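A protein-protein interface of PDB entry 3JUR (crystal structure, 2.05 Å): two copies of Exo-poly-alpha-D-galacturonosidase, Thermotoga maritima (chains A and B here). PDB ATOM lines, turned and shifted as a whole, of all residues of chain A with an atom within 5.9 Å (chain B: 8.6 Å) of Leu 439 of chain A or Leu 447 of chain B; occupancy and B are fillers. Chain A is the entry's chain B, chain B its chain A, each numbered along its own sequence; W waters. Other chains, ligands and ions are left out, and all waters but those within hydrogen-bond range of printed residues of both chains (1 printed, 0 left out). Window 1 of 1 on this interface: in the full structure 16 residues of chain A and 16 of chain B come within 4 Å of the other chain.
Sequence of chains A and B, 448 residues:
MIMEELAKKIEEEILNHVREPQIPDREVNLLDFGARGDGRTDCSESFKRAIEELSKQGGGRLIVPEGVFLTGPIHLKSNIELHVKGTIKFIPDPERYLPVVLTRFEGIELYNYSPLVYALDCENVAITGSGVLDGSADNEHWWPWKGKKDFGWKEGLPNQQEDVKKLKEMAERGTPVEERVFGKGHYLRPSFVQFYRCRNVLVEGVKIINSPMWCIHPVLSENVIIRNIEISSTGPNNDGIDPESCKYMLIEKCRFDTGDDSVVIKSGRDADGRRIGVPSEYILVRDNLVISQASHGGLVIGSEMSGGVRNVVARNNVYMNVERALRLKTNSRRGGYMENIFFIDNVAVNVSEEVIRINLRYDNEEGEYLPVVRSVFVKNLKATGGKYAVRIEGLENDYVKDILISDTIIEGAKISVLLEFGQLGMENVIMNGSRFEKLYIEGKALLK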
ATOM      1  N   VAL A 417      -4.646  -1.670  -8.119  1.00  0.00           N
ATOM      2  CA  VAL A 417      -4.409  -0.622  -7.135  1.00  0.00           C
ATOM      3  C   VAL A 417      -2.928  -0.526  -6.817  1.00  0.00           C
ATOM      4  O   VAL A 417      -2.292  -1.523  -6.490  1.00  0.00           O
ATOM      5  CB  VAL A 417      -5.192  -0.868  -5.814  1.00  0.00           C
ATOM      6  CG1 VAL A 417      -4.889   0.233  -4.793  1.00  0.00           C
ATOM      7  CG2 VAL A 417      -6.720  -0.974  -6.069  1.00  0.00           C
ATOM      8  N   LEU A 424      -7.793   4.547   1.060  1.00  0.00           N
ATOM      9  CA  LEU A 424      -8.685   4.204  -0.035  1.00  0.00           C
ATOM     10  C   LEU A 424      -9.848   3.333   0.432  1.00  0.00           C
ATOM     11  O   LEU A 424      -9.649   2.327   1.120  1.00  0.00           O
ATOM     12  CB  LEU A 424      -7.909   3.498  -1.160  1.00  0.00           C
ATOM     13  CG  LEU A 424      -8.670   3.030  -2.411  1.00  0.00           C
ATOM     14  CD1 LEU A 424      -9.222   4.221  -3.203  1.00  0.00           C
ATOM     15  CD2 LEU A 424      -7.773   2.152  -3.288  1.00  0.00           C
ATOM     16  N   GLY A 425     -11.060   3.740   0.054  1.00  0.00           N
ATOM     17  CA  GLY A 425     -12.261   2.927   0.227  1.00  0.00           C
ATOM     18  C   GLY A 425     -12.832   2.550  -1.127  1.00  0.00           C
ATOM     19  O   GLY A 425     -12.866   3.379  -2.037  1.00  0.00           O
ATOM     20  N   MET A 426     -13.252   1.294  -1.276  1.00  0.00           N
ATOM     21  CA  MET A 426     -13.971   0.852  -2.478  1.00  0.00           C
ATOM     22  C   MET A 426     -15.186   0.055  -2.053  1.00  0.00           C
ATOM     23  O   MET A 426     -15.083  -0.825  -1.191  1.00  0.00           O
ATOM     24  CB  MET A 426     -13.096   0.020  -3.434  1.00  0.00           C
ATOM     25  CG  MET A 426     -11.807   0.711  -3.868  1.00  0.00           C
ATOM     26  SD  MET A 426     -11.012   0.127  -5.382  1.00  0.00           S
ATOM     27  CE  MET A 426     -10.302  -1.429  -4.881  1.00  0.00           C
ATOM     28  N   GLU A 427     -16.337   0.389  -2.639  1.00  0.00           N
ATOM     29  CA  GLU A 427     -17.592  -0.319  -2.369  1.00  0.00           C
ATOM     30  C   GLU A 427     -18.266  -0.682  -3.684  1.00  0.00           C
ATOM     31  O   GLU A 427     -18.513   0.194  -4.524  1.00  0.00           O
ATOM     32  CB  GLU A 427     -18.529   0.527  -1.508  1.00  0.00           C
ATOM     33  CG  GLU A 427     -17.932   0.910  -0.158  1.00  0.00           C
ATOM     34  CD  GLU A 427     -18.692   2.015   0.557  1.00  0.00           C
ATOM     35  OE1 GLU A 427     -19.626   2.610  -0.027  1.00  0.00           O
ATOM     36  OE2 GLU A 427     -18.340   2.298   1.716  1.00  0.00           O
ATOM     37  N   PHE A 436     -14.698  -6.278  -5.194  1.00  0.00           N
ATOM     38  CA  PHE A 436     -14.641  -5.689  -3.868  1.00  0.00           C
ATOM     39  C   PHE A 436     -16.035  -5.230  -3.462  1.00  0.00           C
ATOM     40  O   PHE A 436     -16.514  -4.192  -3.934  1.00  0.00           O
ATOM     41  CB  PHE A 436     -13.651  -4.509  -3.841  1.00  0.00           C
ATOM     42  CG  PHE A 436     -12.331  -4.799  -4.521  1.00  0.00           C
ATOM     43  CD1 PHE A 436     -11.297  -5.423  -3.831  1.00  0.00           C
ATOM     44  CD2 PHE A 436     -12.125  -4.444  -5.854  1.00  0.00           C
ATOM     45  CE1 PHE A 436     -10.076  -5.694  -4.454  1.00  0.00           C
ATOM     46  CE2 PHE A 436     -10.901  -4.709  -6.491  1.00  0.00           C
ATOM     47  CZ  PHE A 436      -9.876  -5.337  -5.786  1.00  0.00           C
ATOM     48  N   GLU A 437     -16.693  -6.017  -2.613  1.00  0.00           N
ATOM     49  CA  GLU A 437     -17.945  -5.580  -2.000  1.00  0.00           C
ATOM     50  C   GLU A 437     -17.649  -4.385  -1.098  1.00  0.00           C
ATOM     51  O   GLU A 437     -18.319  -3.348  -1.183  1.00  0.00           O
ATOM     52  CB  GLU A 437     -18.605  -6.698  -1.190  1.00  0.00           C
ATOM     53  CG  GLU A 437     -19.935  -6.268  -0.554  1.00  0.00           C
ATOM     54  CD  GLU A 437     -20.503  -7.303   0.400  1.00  0.00           C
ATOM     55  OE1 GLU A 437     -20.370  -8.515   0.121  1.00  0.00           O
ATOM     56  OE2 GLU A 437     -21.089  -6.899   1.429  1.00  0.00           O
ATOM     57  N   LYS A 438     -16.633  -4.538  -0.248  1.00  0.00           N
ATOM     58  CA  LYS A 438     -16.175  -3.456   0.602  1.00  0.00           C
ATOM     59  C   LYS A 438     -14.696  -3.608   0.938  1.00  0.00           C
ATOM     60  O   LYS A 438     -14.287  -4.579   1.581  1.00  0.00           O
ATOM     61  CB  LYS A 438     -17.026  -3.358   1.871  1.00  0.00           C
ATOM     62  CG  LYS A 438     -16.825  -2.054   2.622  1.00  0.00           C
ATOM     63  CD  LYS A 438     -17.880  -1.841   3.689  1.00  0.00           C
ATOM     64  CE  LYS A 438     -17.600  -0.538   4.416  1.00  0.00           C
ATOM     65  NZ  LYS A 438     -18.850   0.203   4.762  1.00  0.00           N
ATOM     66  N   LEU A 439     -13.905  -2.652   0.467  1.00  0.00           N
ATOM     67  CA  LEU A 439     -12.471  -2.592   0.735  1.00  0.00           C
ATOM     68  C   LEU A 439     -12.145  -1.262   1.406  1.00  0.00           C
ATOM     69  O   LEU A 439     -12.641  -0.211   1.000  1.00  0.00           O
ATOM     70  CB  LEU A 439     -11.671  -2.708  -0.570  1.00  0.00           C
ATOM     71  CG  LEU A 439     -10.157  -2.446  -0.571  1.00  0.00           C
ATOM     72  CD1 LEU A 439      -9.466  -3.234  -1.667  1.00  0.00           C
ATOM     73  CD2 LEU A 439      -9.837  -0.961  -0.730  1.00  0.00           C
ATOM     74  N   TYR A 440     -11.308  -1.326   2.435  1.00  0.00           N
ATOM     75  CA  TYR A 440     -10.709  -0.143   3.008  1.00  0.00           C
ATOM     76  C   TYR A 440      -9.233  -0.418   3.254  1.00  0.00           C
ATOM     77  O   TYR A 440      -8.889  -1.417   3.886  1.00  0.00           O
ATOM     78  CB  TYR A 440     -11.413   0.274   4.312  1.00  0.00           C
ATOM     79  CG  TYR A 440     -10.684   1.390   5.032  1.00  0.00           C
ATOM     80  CD1 TYR A 440     -10.794   2.722   4.601  1.00  0.00           C
ATOM     81  CD2 TYR A 440      -9.853   1.115   6.125  1.00  0.00           C
ATOM     82  CE1 TYR A 440     -10.110   3.749   5.252  1.00  0.00           C
ATOM     83  CE2 TYR A 440      -9.164   2.134   6.782  1.00  0.00           C
ATOM     84  CZ  TYR A 440      -9.296   3.443   6.341  1.00  0.00           C
ATOM     85  OH  TYR A 440      -8.610   4.445   6.994  1.00  0.00           O
ATOM     86  N   ILE A 441      -8.364   0.454   2.749  1.00  0.00           N
ATOM     87  CA  ILE A 441      -6.925   0.353   3.022  1.00  0.00           C
ATOM     88  C   ILE A 441      -6.351   1.720   3.432  1.00  0.00           C
ATOM     89  O   ILE A 441      -6.674   2.755   2.831  1.00  0.00           O
ATOM     90  CB  ILE A 441      -6.112  -0.217   1.823  1.00  0.00           C
ATOM     91  CG1 ILE A 441      -6.632  -1.599   1.390  1.00  0.00           C
ATOM     92  CG2 ILE A 441      -4.617  -0.313   2.190  1.00  0.00           C
ATOM     93  CD1 ILE A 441      -6.063  -2.097   0.053  1.00  0.00           C
ATOM     94  N   LEU A 447      -2.220  -4.184  -5.559  1.00  0.00           N
ATOM     95  CA  LEU A 447      -3.196  -5.196  -5.936  1.00  0.00           C
ATOM     96  C   LEU A 447      -3.138  -5.412  -7.444  1.00  0.00           C
ATOM     97  O   LEU A 447      -3.302  -4.464  -8.227  1.00  0.00           O
ATOM     98  CB  LEU A 447      -4.609  -4.759  -5.524  1.00  0.00           C
ATOM     99  CG  LEU A 447      -5.166  -5.001  -4.113  1.00  0.00           C
ATOM    100  CD1 LEU A 447      -4.309  -4.425  -2.997  1.00  0.00           C
ATOM    101  CD2 LEU A 447      -6.577  -4.407  -4.028  1.00  0.00           C
ATOM    102  N   LYS B 387     -15.682 -16.806   9.612  1.00  0.00           N
ATOM    103  CA  LYS B 387     -16.086 -15.424   9.731  1.00  0.00           C
ATOM    104  C   LYS B 387     -15.007 -14.546   9.105  1.00  0.00           C
ATOM    105  O   LYS B 387     -15.317 -13.512   8.513  1.00  0.00           O
ATOM    106  CB  LYS B 387     -16.319 -15.062  11.198  1.00  0.00           C
ATOM    107  CG  LYS B 387     -17.609 -15.670  11.758  1.00  0.00           C
ATOM    108  CD  LYS B 387     -17.663 -15.561  13.273  1.00  0.00           C
ATOM    109  CE  LYS B 387     -18.983 -16.108  13.813  1.00  0.00           C
ATOM    110  NZ  LYS B 387     -18.838 -16.448  15.252  1.00  0.00           N
ATOM    111  N   TYR B 388     -13.749 -14.973   9.234  1.00  0.00           N
ATOM    112  CA  TYR B 388     -12.622 -14.338   8.552  1.00  0.00           C
ATOM    113  C   TYR B 388     -11.811 -15.379   7.797  1.00  0.00           C
ATOM    114  O   TYR B 388     -11.579 -16.479   8.297  1.00  0.00           O
ATOM    115  CB  TYR B 388     -11.693 -13.628   9.553  1.00  0.00           C
ATOM    116  CG  TYR B 388     -12.345 -12.507  10.325  1.00  0.00           C
ATOM    117  CD1 TYR B 388     -12.160 -11.183   9.945  1.00  0.00           C
ATOM    118  CD2 TYR B 388     -13.149 -12.772  11.439  1.00  0.00           C
ATOM    119  CE1 TYR B 388     -12.771 -10.143  10.649  1.00  0.00           C
ATOM    120  CE2 TYR B 388     -13.752 -11.740  12.156  1.00  0.00           C
ATOM    121  CZ  TYR B 388     -13.561 -10.430  11.752  1.00  0.00           C
ATOM    122  OH  TYR B 388     -14.158  -9.402  12.446  1.00  0.00           O
ATOM    123  N   ALA B 389     -11.372 -15.033   6.593  1.00  0.00           N
ATOM    124  CA  ALA B 389     -10.367 -15.836   5.902  1.00  0.00           C
ATOM    125  C   ALA B 389      -8.999 -15.570   6.532  1.00  0.00           C
ATOM    126  O   ALA B 389      -8.299 -16.488   6.954  1.00  0.00           O
ATOM    127  CB  ALA B 389     -10.354 -15.512   4.404  1.00  0.00           C
ATOM    128  N   VAL B 390      -8.633 -14.292   6.603  1.00  0.00           N
ATOM    129  CA  VAL B 390      -7.352 -13.877   7.159  1.00  0.00           C
ATOM    130  C   VAL B 390      -7.580 -12.725   8.139  1.00  0.00           C
ATOM    131  O   VAL B 390      -8.146 -11.688   7.775  1.00  0.00           O
ATOM    132  CB  VAL B 390      -6.364 -13.399   6.055  1.00  0.00           C
ATOM    133  CG1 VAL B 390      -5.059 -12.908   6.675  1.00  0.00           C
ATOM    134  CG2 VAL B 390      -6.098 -14.500   5.010  1.00  0.00           C
ATOM    135  N   ALA B 413     -15.841 -17.644   3.241  1.00  0.00           N
ATOM    136  CA  ALA B 413     -15.550 -16.847   4.435  1.00  0.00           C
ATOM    137  C   ALA B 413     -16.281 -15.523   4.309  1.00  0.00           C
ATOM    138  O   ALA B 413     -16.370 -14.990   3.218  1.00  0.00           O
ATOM    139  CB  ALA B 413     -14.068 -16.621   4.579  1.00  0.00           C
ATOM    140  N   LYS B 414     -16.805 -14.988   5.410  1.00  0.00           N
ATOM    141  CA  LYS B 414     -17.567 -13.737   5.345  1.00  0.00           C
ATOM    142  C   LYS B 414     -16.649 -12.547   5.023  1.00  0.00           C
ATOM    143  O   LYS B 414     -16.880 -11.820   4.053  1.00  0.00           O
ATOM    144  CB  LYS B 414     -18.359 -13.508   6.637  1.00  0.00           C
ATOM    145  CG  LYS B 414     -19.601 -12.629   6.451  1.00  0.00           C
ATOM    146  CD  LYS B 414     -20.538 -12.659   7.672  1.00  0.00           C
ATOM    147  CE  LYS B 414     -21.296 -13.996   7.827  1.00  0.00           C
ATOM    148  NZ  LYS B 414     -20.619 -14.969   8.759  1.00  0.00           N
ATOM    149  N   ILE B 415     -15.606 -12.368   5.826  1.00  0.00           N
ATOM    150  CA  ILE B 415     -14.625 -11.327   5.595  1.00  0.00           C
ATOM    151  C   ILE B 415     -13.359 -11.982   5.033  1.00  0.00           C
ATOM    152  O   ILE B 415     -12.938 -13.034   5.510  1.00  0.00           O
ATOM    153  CB  ILE B 415     -14.346 -10.523   6.890  1.00  0.00           C
ATOM    154  CG1 ILE B 415     -15.590  -9.719   7.278  1.00  0.00           C
ATOM    155  CG2 ILE B 415     -13.151  -9.576   6.718  1.00  0.00           C
ATOM    156  CD1 ILE B 415     -15.496  -9.034   8.632  1.00  0.00           C
ATOM    157  N   SER B 416     -12.785 -11.372   4.000  1.00  0.00           N
ATOM    158  CA  SER B 416     -11.569 -11.902   3.379  1.00  0.00           C
ATOM    159  C   SER B 416     -10.323 -11.531   4.169  1.00  0.00           C
ATOM    160  O   SER B 416      -9.577 -12.399   4.588  1.00  0.00           O
ATOM    161  CB  SER B 416     -11.446 -11.424   1.929  1.00  0.00           C
ATOM    162  OG  SER B 416     -12.433 -12.037   1.138  1.00  0.00           O
ATOM    163  N   VAL B 417     -10.100 -10.237   4.357  1.00  0.00           N
ATOM    164  CA  VAL B 417      -8.933  -9.764   5.085  1.00  0.00           C
ATOM    165  C   VAL B 417      -9.320  -8.717   6.134  1.00  0.00           C
ATOM    166  O   VAL B 417      -9.972  -7.713   5.818  1.00  0.00           O
ATOM    167  CB  VAL B 417      -7.846  -9.173   4.126  1.00  0.00           C
ATOM    168  CG1 VAL B 417      -6.663  -8.620   4.921  1.00  0.00           C
ATOM    169  CG2 VAL B 417      -7.353 -10.215   3.117  1.00  0.00           C
ATOM    170  N   LEU B 418      -8.936  -8.976   7.383  1.00  0.00           N
ATOM    171  CA  LEU B 418      -8.853  -7.931   8.406  1.00  0.00           C
ATOM    172  C   LEU B 418      -7.382  -7.805   8.781  1.00  0.00           C
ATOM    173  O   LEU B 418      -6.762  -8.766   9.255  1.00  0.00           O
ATOM    174  CB  LEU B 418      -9.715  -8.255   9.635  1.00  0.00           C
ATOM    175  CG  LEU B 418      -9.776  -7.214  10.767  1.00  0.00           C
ATOM    176  CD1 LEU B 418     -11.002  -7.429  11.640  1.00  0.00           C
ATOM    177  CD2 LEU B 418      -8.534  -7.241  11.650  1.00  0.00           C
ATOM    178  N   LEU B 419      -6.820  -6.623   8.540  1.00  0.00           N
ATOM    179  CA  LEU B 419      -5.421  -6.357   8.849  1.00  0.00           C
ATOM    180  C   LEU B 419      -5.294  -5.063   9.661  1.00  0.00           C
ATOM    181  O   LEU B 419      -5.889  -4.038   9.311  1.00  0.00           O
ATOM    182  CB  LEU B 419      -4.601  -6.271   7.558  1.00  0.00           C
ATOM    183  CG  LEU B 419      -3.107  -5.931   7.640  1.00  0.00           C
ATOM    184  CD1 LEU B 419      -2.291  -7.051   8.317  1.00  0.00           C
ATOM    185  CD2 LEU B 419      -2.578  -5.649   6.245  1.00  0.00           C
ATOM    186  N   LEU B 424       1.313  -7.774   4.944  1.00  0.00           N
ATOM    187  CA  LEU B 424       0.756  -8.995   4.372  1.00  0.00           C
ATOM    188  C   LEU B 424       1.056  -9.047   2.887  1.00  0.00           C
ATOM    189  O   LEU B 424       0.765  -8.096   2.159  1.00  0.00           O
ATOM    190  CB  LEU B 424      -0.764  -9.068   4.610  1.00  0.00           C
ATOM    191  CG  LEU B 424      -1.586 -10.182   3.937  1.00  0.00           C
ATOM    192  CD1 LEU B 424      -1.295 -11.570   4.526  1.00  0.00           C
ATOM    193  CD2 LEU B 424      -3.078  -9.881   4.043  1.00  0.00           C
ATOM    194  N   MET B 426       0.394 -11.533  -0.584  1.00  0.00           N
ATOM    195  CA  MET B 426      -0.287 -12.689  -1.157  1.00  0.00           C
ATOM    196  C   MET B 426       0.084 -12.843  -2.624  1.00  0.00           C
ATOM    197  O   MET B 426       0.166 -11.855  -3.362  1.00  0.00           O
ATOM    198  CB  MET B 426      -1.808 -12.595  -0.972  1.00  0.00           C
ATOM    199  CG  MET B 426      -2.251 -12.353   0.474  1.00  0.00           C
ATOM    200  SD  MET B 426      -4.041 -12.402   0.714  1.00  0.00           S
ATOM    201  CE  MET B 426      -4.312 -14.174   0.682  1.00  0.00           C
ATOM    202  N   MET B 431      -9.817 -15.617  -3.073  1.00  0.00           N
ATOM    203  CA  MET B 431     -10.619 -15.414  -1.873  1.00  0.00           C
ATOM    204  C   MET B 431     -12.053 -15.082  -2.229  1.00  0.00           C
ATOM    205  O   MET B 431     -12.323 -14.040  -2.837  1.00  0.00           O
ATOM    206  CB  MET B 431     -10.013 -14.310  -1.017  1.00  0.00           C
ATOM    207  CG  MET B 431      -8.875 -14.807  -0.131  1.00  0.00           C
ATOM    208  SD  MET B 431      -8.126 -13.436   0.744  1.00  0.00           S
ATOM    209  CE  MET B 431      -7.401 -14.340   2.088  1.00  0.00           C
ATOM    210  N   ASN B 432     -12.963 -15.982  -1.856  1.00  0.00           N
ATOM    211  CA  ASN B 432     -14.386 -15.868  -2.180  1.00  0.00           C
ATOM    212  C   ASN B 432     -14.632 -15.508  -3.641  1.00  0.00           C
ATOM    213  O   ASN B 432     -15.389 -14.583  -3.930  1.00  0.00           O
ATOM    214  CB  ASN B 432     -15.081 -14.839  -1.285  1.00  0.00           C
ATOM    215  CG  ASN B 432     -15.114 -15.243   0.169  1.00  0.00           C
ATOM    216  OD1 ASN B 432     -15.061 -16.427   0.521  1.00  0.00           O
ATOM    217  ND2 ASN B 432     -15.208 -14.247   1.034  1.00  0.00           N
ATOM    218  N   SER B 434     -12.657 -14.006  -5.728  1.00  0.00           N
ATOM    219  CA  SER B 434     -11.802 -12.928  -6.223  1.00  0.00           C
ATOM    220  C   SER B 434     -10.385 -13.440  -6.358  1.00  0.00           C
ATOM    221  O   SER B 434      -9.838 -14.031  -5.415  1.00  0.00           O
ATOM    222  CB  SER B 434     -11.794 -11.734  -5.278  1.00  0.00           C
ATOM    223  OG  SER B 434     -12.816 -10.842  -5.610  1.00  0.00           O
ATOM    224  N   PHE B 436      -6.360 -12.821  -7.015  1.00  0.00           N
ATOM    225  CA  PHE B 436      -5.264 -11.870  -6.914  1.00  0.00           C
ATOM    226  C   PHE B 436      -3.977 -12.549  -7.340  1.00  0.00           C
ATOM    227  O   PHE B 436      -3.564 -13.538  -6.724  1.00  0.00           O
ATOM    228  CB  PHE B 436      -5.114 -11.350  -5.479  1.00  0.00           C
ATOM    229  CG  PHE B 436      -6.297 -10.571  -4.994  1.00  0.00           C
ATOM    230  CD1 PHE B 436      -6.469  -9.242  -5.372  1.00  0.00           C
ATOM    231  CD2 PHE B 436      -7.239 -11.163  -4.157  1.00  0.00           C
ATOM    232  CE1 PHE B 436      -7.577  -8.512  -4.935  1.00  0.00           C
ATOM    233  CE2 PHE B 436      -8.346 -10.450  -3.708  1.00  0.00           C
ATOM    234  CZ  PHE B 436      -8.521  -9.118  -4.102  1.00  0.00           C
ATOM    235  N   LEU B 439      -1.342  -9.431  -3.971  1.00  0.00           N
ATOM    236  CA  LEU B 439      -1.995  -8.544  -3.022  1.00  0.00           C
ATOM    237  C   LEU B 439      -1.001  -8.284  -1.898  1.00  0.00           C
ATOM    238  O   LEU B 439      -0.718  -9.177  -1.089  1.00  0.00           O
ATOM    239  CB  LEU B 439      -3.311  -9.136  -2.476  1.00  0.00           C
ATOM    240  CG  LEU B 439      -4.089  -8.314  -1.423  1.00  0.00           C
ATOM    241  CD1 LEU B 439      -5.567  -8.585  -1.488  1.00  0.00           C
ATOM    242  CD2 LEU B 439      -3.580  -8.571  -0.006  1.00  0.00           C
ATOM    243  N   ILE B 441      -0.176  -5.589   1.238  1.00  0.00           N
ATOM    244  CA  ILE B 441      -0.664  -4.493   2.063  1.00  0.00           C
ATOM    245  C   ILE B 441       0.209  -4.289   3.295  1.00  0.00           C
ATOM    246  O   ILE B 441       0.560  -5.248   3.989  1.00  0.00           O
ATOM    247  CB  ILE B 441      -2.153  -4.676   2.504  1.00  0.00           C
ATOM    248  CG1 ILE B 441      -3.061  -5.017   1.312  1.00  0.00           C
ATOM    249  CG2 ILE B 441      -2.667  -3.395   3.201  1.00  0.00           C
ATOM    250  CD1 ILE B 441      -4.524  -5.289   1.685  1.00  0.00           C
ATOM    251  N   LYS B 444      -3.181  -0.853   7.637  1.00  0.00           N
ATOM    252  CA  LYS B 444      -4.518  -1.325   8.018  1.00  0.00           C
ATOM    253  C   LYS B 444      -5.359  -1.645   6.777  1.00  0.00           C
ATOM    254  O   LYS B 444      -5.270  -0.942   5.754  1.00  0.00           O
ATOM    255  CB  LYS B 444      -5.268  -0.254   8.823  1.00  0.00           C
ATOM    256  CG  LYS B 444      -4.628   0.206  10.143  1.00  0.00           C
ATOM    257  CD  LYS B 444      -5.478   1.344  10.725  1.00  0.00           C
ATOM    258  CE  LYS B 444      -5.379   1.428  12.239  1.00  0.00           C
ATOM    259  NZ  LYS B 444      -4.351   2.391  12.691  1.00  0.00           N
ATOM    260  N   ALA B 445      -6.196  -2.674   6.880  1.00  0.00           N
ATOM    261  CA  ALA B 445      -7.123  -3.041   5.803  1.00  0.00           C
ATOM    262  C   ALA B 445      -8.331  -3.846   6.291  1.00  0.00           C
ATOM    263  O   ALA B 445      -8.242  -4.631   7.246  1.00  0.00           O
ATOM    264  CB  ALA B 445      -6.395  -3.812   4.696  1.00  0.00           C
ATOM    265  N   LEU B 446      -9.452  -3.634   5.615  1.00  0.00           N
ATOM    266  CA  LEU B 446     -10.627  -4.465   5.767  1.00  0.00           C
ATOM    267  C   LEU B 446     -11.181  -4.760   4.375  1.00  0.00           C
ATOM    268  O   LEU B 446     -11.587  -3.831   3.665  1.00  0.00           O
ATOM    269  CB  LEU B 446     -11.677  -3.781   6.649  1.00  0.00           C
ATOM    270  CG  LEU B 446     -12.970  -4.569   6.922  1.00  0.00           C
ATOM    271  CD1 LEU B 446     -12.698  -5.917   7.585  1.00  0.00           C
ATOM    272  CD2 LEU B 446     -13.938  -3.740   7.770  1.00  0.00           C
ATOM    273  N   LEU B 447     -11.155  -6.037   3.980  1.00  0.00           N
ATOM    274  CA  LEU B 447     -11.645  -6.476   2.663  1.00  0.00           C
ATOM    275  C   LEU B 447     -12.765  -7.509   2.765  1.00  0.00           C
ATOM    276  O   LEU B 447     -12.596  -8.583   3.370  1.00  0.00           O
ATOM    277  CB  LEU B 447     -10.539  -7.080   1.786  1.00  0.00           C
ATOM    278  CG  LEU B 447      -9.132  -6.524   1.527  1.00  0.00           C
ATOM    279  CD1 LEU B 447      -8.882  -6.653   0.035  1.00  0.00           C
ATOM    280  CD2 LEU B 447      -8.875  -5.091   1.990  1.00  0.00           C
ATOM    281  N   LYS B 448     -13.891  -7.169   2.144  1.00  0.00           N
ATOM    282  CA  LYS B 448     -15.062  -8.034   2.052  1.00  0.00           C
ATOM    283  C   LYS B 448     -15.431  -8.199   0.572  1.00  0.00           C
ATOM    284  O   LYS B 448     -15.416  -7.236  -0.207  1.00  0.00           O
ATOM    285  CB  LYS B 448     -16.230  -7.397   2.814  1.00  0.00           C
ATOM    286  CG  LYS B 448     -17.392  -8.318   3.108  1.00  0.00           C
ATOM    287  CD  LYS B 448     -18.507  -7.567   3.832  1.00  0.00           C
ATOM    288  CE  LYS B 448     -19.412  -8.519   4.608  1.00  0.00           C
ATOM    289  NZ  LYS B 448     -20.050  -9.558   3.742  1.00  0.00           N
ATOM    290  OXT LYS B 448     -15.763  -9.290   0.104  1.00  0.00           O
HETATM  291  O   HOH W   1     -15.809  -9.364  -2.636  1.00  0.00           O
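The backbone NH of Ser 416 of chain B is in hydrogen-bond range of the backbone carbonyl oxygen of Leu 447 of chain B, at 2.9 Å.
N of Leu 447 of chain B lies within hydrogen-bond range of O of Val 417 of chain B, at 2.8 Å.
The backbone NH of Leu 419 of chain B is in hydrogen-bond range of the backbone carbonyl oxygen of Ala 445 of chain B, at 2.8 Å.
N of Leu 424 of chain B lies within hydrogen-bond range of O of Ile 441 of chain B, 2.8 Å away.
N of Leu 424 of chain A sits at hydrogen-bond distance from O of Ile 441 of chain A (2.8 Å).
The side-chain amino group (NZ) of Lys 438 of chain A is in salt-bridge range of the side-chain carboxylate (OE2) of Glu 427 of chain A, 3.7 Å away.
Phe 436 of chain A touches its own counterpart, Phe 436 of chain B.
Leu 439 of chain A touches Leu 447 of chain B, but with the chains exchanged Leu 447 of chain A does not touch Leu 439 of chain B (4.2 Å).
Ile 441 of chain A touches its own counterpart, Ile 441 of chain B.
Positions printed for both chains: 417, 424, 426, 436, 439, 441 and 447.
Of the 24 printed residues of chain B, 7 touch a printed residue of chain A.
Printed residues of chain B that touch a printed residue of chain A: Phe 436, Ile 441, Lys 444, Ala 445, Leu 446, Leu 447 and Lys 448.
Hydrophobic or aromatic side chains of chain A within 4 Å of the printed part of chain B: Phe 436, Leu 439 and Ile 441.
Among the printed residues, Asp or Glu carboxylates within 4 Å of a Lys or Arg side-chain nitrogen of the other chain: Glu 437 of chain A with Lys 448 of chain B (3.7 Å).
Water W1 bridges the chain-end carboxylate of Lys 448 of chain B (2.7 Å) and the backbone NH of Glu 437 of chain A (3.5 Å).
The backbone carbonyl oxygen (O) of Leu 446 of chain B lies within hydrogen-bond range of the backbone NH (N) of Tyr 440 of chain A, 2.8 Å away.
The side-chain carboxylate (OE2) of Glu 437 of chain A is in salt-bridge range of the side-chain amino group (NZ) of Lys 448 of chain B.
N of Lys 448 of chain B is in hydrogen-bond range of O of Lys 438 of chain A (2.7 Å).
The backbone carbonyl oxygen (O) of Lys 438 of chain A lies close to the backbone carbonyl oxygen (O) of Leu 446 of chain B (3.5 Å).
Ala 389 of chain B touches none of the printed residues of chain A.
Of the printed residues of chain A, Phe 436 of chain B touches Phe 436 (3.8 Å).
Of the printed residues of chain A, Leu 446 of chain B touches Lys 438, Leu 439 and Tyr 440.
The nearest printed residue of chain B that does not touch Lys 438 of chain A is Val 417 of chain B (6.8 Å).
Among the printed residues, pairs that only touch across the chains: Phe 436 of chain A with Phe 436 of chain B (3.8 Å), Phe 436 of chain A with Lys 448 of chain B (3.9 Å), Lys 438 of chain A with Leu 447 of chain B (3.4 Å), Leu 439 of chain A with Leu 446 of chain B (3.3 Å), Leu 439 of chain A with Leu 447 of chain B (3.9 Å), Tyr 440 of chain A with Ala 445 of chain B (3.1 Å), Ile 441 of chain A with Ile 441 of chain B (3.8 Å), Ile 441 of chain A with Lys 444 of chain B (3.4 Å) and Ile 441 of chain A with Ala 445 of chain B (3.99 Å).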
